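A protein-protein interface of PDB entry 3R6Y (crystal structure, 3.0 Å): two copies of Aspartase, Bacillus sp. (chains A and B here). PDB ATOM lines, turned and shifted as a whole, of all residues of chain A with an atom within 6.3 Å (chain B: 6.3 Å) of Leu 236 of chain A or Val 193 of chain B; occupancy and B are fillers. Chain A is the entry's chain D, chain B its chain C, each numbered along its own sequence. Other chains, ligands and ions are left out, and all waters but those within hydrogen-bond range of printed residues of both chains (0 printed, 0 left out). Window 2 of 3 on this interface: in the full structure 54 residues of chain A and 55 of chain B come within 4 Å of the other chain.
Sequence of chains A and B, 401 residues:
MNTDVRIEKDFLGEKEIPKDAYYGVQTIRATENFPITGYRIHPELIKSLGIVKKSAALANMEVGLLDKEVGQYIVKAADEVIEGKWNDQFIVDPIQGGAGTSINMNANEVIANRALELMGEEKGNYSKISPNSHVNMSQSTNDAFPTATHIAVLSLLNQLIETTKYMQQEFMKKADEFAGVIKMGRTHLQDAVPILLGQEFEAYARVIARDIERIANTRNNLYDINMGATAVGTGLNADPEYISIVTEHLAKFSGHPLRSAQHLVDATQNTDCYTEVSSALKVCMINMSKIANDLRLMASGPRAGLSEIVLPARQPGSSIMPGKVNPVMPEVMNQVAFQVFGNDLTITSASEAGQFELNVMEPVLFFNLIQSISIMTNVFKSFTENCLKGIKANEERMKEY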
ATOM      1  N   GLY A 228       8.678 -18.020 -19.559  1.00  0.00           N
ATOM      2  CA  GLY A 228       9.209 -18.031 -20.922  1.00  0.00           C
ATOM      3  C   GLY A 228       9.052 -19.357 -21.648  1.00  0.00           C
ATOM      4  O   GLY A 228       9.532 -19.509 -22.779  1.00  0.00           O
ATOM      5  N   ALA A 229       8.390 -20.319 -20.999  1.00  0.00           N
ATOM      6  CA  ALA A 229       7.942 -21.542 -21.661  1.00  0.00           C
ATOM      7  C   ALA A 229       6.666 -21.251 -22.448  1.00  0.00           C
ATOM      8  O   ALA A 229       6.217 -22.078 -23.241  1.00  0.00           O
ATOM      9  CB  ALA A 229       7.700 -22.642 -20.649  1.00  0.00           C
ATOM     10  N   THR A 230       6.086 -20.073 -22.217  1.00  0.00           N
ATOM     11  CA  THR A 230       4.946 -19.576 -22.981  1.00  0.00           C
ATOM     12  C   THR A 230       3.861 -20.651 -23.155  1.00  0.00           C
ATOM     13  O   THR A 230       3.336 -21.148 -22.164  1.00  0.00           O
ATOM     14  CB  THR A 230       5.391 -18.980 -24.333  1.00  0.00           C
ATOM     15  OG1 THR A 230       5.964 -20.009 -25.147  1.00  0.00           O
ATOM     16  CG2 THR A 230       6.409 -17.869 -24.118  1.00  0.00           C
ATOM     17  N   ALA A 231       3.545 -21.032 -24.392  1.00  0.00           N
ATOM     18  CA  ALA A 231       2.359 -21.852 -24.663  1.00  0.00           C
ATOM     19  C   ALA A 231       2.543 -23.356 -24.426  1.00  0.00           C
ATOM     20  O   ALA A 231       1.623 -24.012 -23.939  1.00  0.00           O
ATOM     21  CB  ALA A 231       1.869 -21.605 -26.081  1.00  0.00           C
ATOM     22  N   VAL A 232       3.712 -23.900 -24.775  1.00  0.00           N
ATOM     23  CA  VAL A 232       3.946 -25.355 -24.724  1.00  0.00           C
ATOM     24  C   VAL A 232       5.221 -25.768 -23.979  1.00  0.00           C
ATOM     25  O   VAL A 232       5.184 -26.664 -23.139  1.00  0.00           O
ATOM     26  CB  VAL A 232       3.996 -25.954 -26.145  1.00  0.00           C
ATOM     27  CG1 VAL A 232       4.019 -27.476 -26.089  1.00  0.00           C
ATOM     28  CG2 VAL A 232       2.804 -25.482 -26.957  1.00  0.00           C
ATOM     29  N   GLY A 233       6.342 -25.126 -24.290  1.00  0.00           N
ATOM     30  CA  GLY A 233       7.638 -25.507 -23.719  1.00  0.00           C
ATOM     31  C   GLY A 233       8.770 -25.531 -24.738  1.00  0.00           C
ATOM     32  O   GLY A 233       9.944 -25.510 -24.371  1.00  0.00           O
ATOM     33  N   THR A 234       8.421 -25.584 -26.024  1.00  0.00           N
ATOM     34  CA  THR A 234       9.406 -25.453 -27.095  1.00  0.00           C
ATOM     35  C   THR A 234       9.954 -24.022 -27.188  1.00  0.00           C
ATOM     36  O   THR A 234      10.906 -23.768 -27.931  1.00  0.00           O
ATOM     37  CB  THR A 234       8.807 -25.845 -28.464  1.00  0.00           C
ATOM     38  OG1 THR A 234       7.624 -25.076 -28.713  1.00  0.00           O
ATOM     39  CG2 THR A 234       8.466 -27.327 -28.496  1.00  0.00           C
ATOM     40  N   GLY A 235       9.349 -23.099 -26.435  1.00  0.00           N
ATOM     41  CA  GLY A 235       9.740 -21.695 -26.442  1.00  0.00           C
ATOM     42  C   GLY A 235       8.715 -20.898 -27.221  1.00  0.00           C
ATOM     43  O   GLY A 235       8.097 -19.982 -26.677  1.00  0.00           O
ATOM     44  N   LEU A 236       8.531 -21.265 -28.492  1.00  0.00           N
ATOM     45  CA  LEU A 236       7.561 -20.619 -29.377  1.00  0.00           C
ATOM     46  C   LEU A 236       7.847 -19.118 -29.422  1.00  0.00           C
ATOM     47  O   LEU A 236       7.012 -18.295 -29.033  1.00  0.00           O
ATOM     48  CB  LEU A 236       6.125 -20.915 -28.909  1.00  0.00           C
ATOM     49  CG  LEU A 236       4.970 -20.642 -29.875  1.00  0.00           C
ATOM     50  CD1 LEU A 236       5.145 -21.426 -31.161  1.00  0.00           C
ATOM     51  CD2 LEU A 236       3.641 -20.985 -29.225  1.00  0.00           C
ATOM     52  N   ASN A 237       9.055 -18.792 -29.889  1.00  0.00           N
ATOM     53  CA  ASN A 237       9.575 -17.414 -29.985  1.00  0.00           C
ATOM     54  C   ASN A 237      10.145 -16.877 -28.661  1.00  0.00           C
ATOM     55  O   ASN A 237      10.086 -15.671 -28.403  1.00  0.00           O
ATOM     56  CB  ASN A 237       8.521 -16.433 -30.545  1.00  0.00           C
ATOM     57  CG  ASN A 237       7.722 -17.014 -31.707  1.00  0.00           C
ATOM     58  OD1 ASN A 237       8.207 -17.868 -32.458  1.00  0.00           O
ATOM     59  ND2 ASN A 237       6.485 -16.554 -31.853  1.00  0.00           N
ATOM     60  N   ALA A 238      10.720 -17.762 -27.845  1.00  0.00           N
ATOM     61  CA  ALA A 238      11.233 -17.383 -26.522  1.00  0.00           C
ATOM     62  C   ALA A 238      12.687 -16.912 -26.591  1.00  0.00           C
ATOM     63  O   ALA A 238      13.605 -17.736 -26.641  1.00  0.00           O
ATOM     64  CB  ALA A 238      11.101 -18.555 -25.544  1.00  0.00           C
ATOM     65  N   LYS B 183       5.085 -34.850 -33.488  1.00  0.00           N
ATOM     66  CA  LYS B 183       3.658 -35.019 -33.215  1.00  0.00           C
ATOM     67  C   LYS B 183       3.026 -33.676 -32.818  1.00  0.00           C
ATOM     68  O   LYS B 183       3.726 -32.705 -32.534  1.00  0.00           O
ATOM     69  CB  LYS B 183       3.441 -36.058 -32.108  1.00  0.00           C
ATOM     70  CG  LYS B 183       4.259 -35.821 -30.838  1.00  0.00           C
ATOM     71  CD  LYS B 183       3.629 -36.486 -29.618  1.00  0.00           C
ATOM     72  CE  LYS B 183       2.504 -35.634 -29.031  1.00  0.00           C
ATOM     73  NZ  LYS B 183       1.718 -36.335 -27.973  1.00  0.00           N
ATOM     74  N   MET B 184       1.700 -33.629 -32.811  1.00  0.00           N
ATOM     75  CA  MET B 184       0.987 -32.426 -32.433  1.00  0.00           C
ATOM     76  C   MET B 184       0.955 -32.292 -30.908  1.00  0.00           C
ATOM     77  O   MET B 184       0.366 -33.129 -30.215  1.00  0.00           O
ATOM     78  CB  MET B 184      -0.434 -32.472 -32.990  1.00  0.00           C
ATOM     79  CG  MET B 184      -1.271 -31.228 -32.708  1.00  0.00           C
ATOM     80  SD  MET B 184      -0.473 -29.682 -33.169  1.00  0.00           S
ATOM     81  CE  MET B 184      -0.228 -29.924 -34.919  1.00  0.00           C
ATOM     82  N   GLY B 185       1.604 -31.250 -30.385  1.00  0.00           N
ATOM     83  CA  GLY B 185       1.518 -30.928 -28.967  1.00  0.00           C
ATOM     84  C   GLY B 185       0.123 -30.413 -28.670  1.00  0.00           C
ATOM     85  O   GLY B 185      -0.453 -29.686 -29.488  1.00  0.00           O
ATOM     86  N   ARG B 186      -0.426 -30.798 -27.515  1.00  0.00           N
ATOM     87  CA  ARG B 186      -1.802 -30.442 -27.141  1.00  0.00           C
ATOM     88  C   ARG B 186      -1.934 -29.860 -25.731  1.00  0.00           C
ATOM     89  O   ARG B 186      -1.404 -30.416 -24.767  1.00  0.00           O
ATOM     90  CB  ARG B 186      -2.692 -31.679 -27.213  1.00  0.00           C
ATOM     91  CG  ARG B 186      -2.705 -32.387 -28.540  1.00  0.00           C
ATOM     92  CD  ARG B 186      -3.613 -33.602 -28.460  1.00  0.00           C
ATOM     93  NE  ARG B 186      -3.710 -34.308 -29.731  1.00  0.00           N
ATOM     94  CZ  ARG B 186      -2.786 -35.129 -30.215  1.00  0.00           C
ATOM     95  NH1 ARG B 186      -1.662 -35.363 -29.546  1.00  0.00           N
ATOM     96  NH2 ARG B 186      -2.981 -35.717 -31.383  1.00  0.00           N
ATOM     97  N   ASP B 191      -5.433 -28.555 -30.216  1.00  0.00           N
ATOM     98  CA  ASP B 191      -4.161 -28.489 -30.922  1.00  0.00           C
ATOM     99  C   ASP B 191      -3.409 -27.209 -30.576  1.00  0.00           C
ATOM    100  O   ASP B 191      -3.952 -26.106 -30.693  1.00  0.00           O
ATOM    101  CB  ASP B 191      -4.362 -28.589 -32.438  1.00  0.00           C
ATOM    102  CG  ASP B 191      -4.867 -29.956 -32.877  1.00  0.00           C
ATOM    103  OD1 ASP B 191      -5.162 -30.085 -34.079  1.00  0.00           O
ATOM    104  OD2 ASP B 191      -4.987 -30.893 -32.044  1.00  0.00           O
ATOM    105  N   ALA B 192      -2.164 -27.371 -30.135  1.00  0.00           N
ATOM    106  CA  ALA B 192      -1.290 -26.246 -29.825  1.00  0.00           C
ATOM    107  C   ALA B 192      -0.365 -26.032 -31.017  1.00  0.00           C
ATOM    108  O   ALA B 192      -0.796 -25.526 -32.049  1.00  0.00           O
ATOM    109  CB  ALA B 192      -0.505 -26.529 -28.548  1.00  0.00           C
ATOM    110  N   VAL B 193       0.899 -26.425 -30.875  1.00  0.00           N
ATOM    111  CA  VAL B 193       1.835 -26.479 -31.988  1.00  0.00           C
ATOM    112  C   VAL B 193       2.494 -27.862 -31.990  1.00  0.00           C
ATOM    113  O   VAL B 193       2.395 -28.607 -31.011  1.00  0.00           O
ATOM    114  CB  VAL B 193       2.937 -25.405 -31.861  1.00  0.00           C
ATOM    115  CG1 VAL B 193       2.338 -24.044 -31.509  1.00  0.00           C
ATOM    116  CG2 VAL B 193       3.983 -25.829 -30.824  1.00  0.00           C
ATOM    117  N   PRO B 194       3.172 -28.219 -33.088  1.00  0.00           N
ATOM    118  CA  PRO B 194       3.870 -29.500 -33.064  1.00  0.00           C
ATOM    119  C   PRO B 194       5.094 -29.454 -32.163  1.00  0.00           C
ATOM    120  O   PRO B 194       5.792 -28.440 -32.133  1.00  0.00           O
ATOM    121  CB  PRO B 194       4.262 -29.709 -34.534  1.00  0.00           C
ATOM    122  CG  PRO B 194       3.272 -28.868 -35.297  1.00  0.00           C
ATOM    123  CD  PRO B 194       3.139 -27.650 -34.448  1.00  0.00           C
ATOM    124  N   ILE B 195       5.306 -30.537 -31.415  1.00  0.00           N
ATOM    125  CA  ILE B 195       6.514 -30.751 -30.601  1.00  0.00           C
ATOM    126  C   ILE B 195       7.113 -32.112 -30.971  1.00  0.00           C
ATOM    127  O   ILE B 195       6.600 -32.796 -31.851  1.00  0.00           O
ATOM    128  CB  ILE B 195       6.216 -30.696 -29.067  1.00  0.00           C
ATOM    129  CG1 ILE B 195       5.455 -31.947 -28.594  1.00  0.00           C
ATOM    130  CG2 ILE B 195       5.423 -29.438 -28.713  1.00  0.00           C
ATOM    131  CD1 ILE B 195       5.420 -32.101 -27.083  1.00  0.00           C
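Among the printed residues, merely in contact across the chains: Val 232 of chain A with Ala 192 of chain B (3.8 Å), Val 232 of chain A with Ile 195 of chain B (3.6 Å), Thr 234 of chain A with Ile 195 of chain B (3.7 Å) and Leu 236 of chain A with Val 193 of chain B (3.9 Å).
No position is printed for both chains. Of the 4 pairs that touch across the chains among the printed residues, none has its exchanged pair printed and touching as well.
Among the printed residues, 4 pairs touch across the chains.
O of Lys 183 of chain B sits at hydrogen-bond distance from N of Ile 195 of chain B. The backbone carbonyl oxygen of Gly 185 of chain B sits at hydrogen-bond distance from the backbone NH of Ala 192 of chain B (3.0 Å). The backbone NH (N) of Gly 185 of chain B sits at hydrogen-bond distance from the backbone carbonyl oxygen (O) of Val 193 of chain B.
Of chain B, only Val 193 comes within 4 Å of Leu 236 of chain A. Printed residues of chain A within 4 Å of Ala 192 of chain B: Val 232 (3.8 Å). Of chain A, only Leu 236 comes within 4 Å of Val 193 of chain B. Of the printed residues of chain A, Ile 195 of chain B touches Val 232 and Thr 234.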
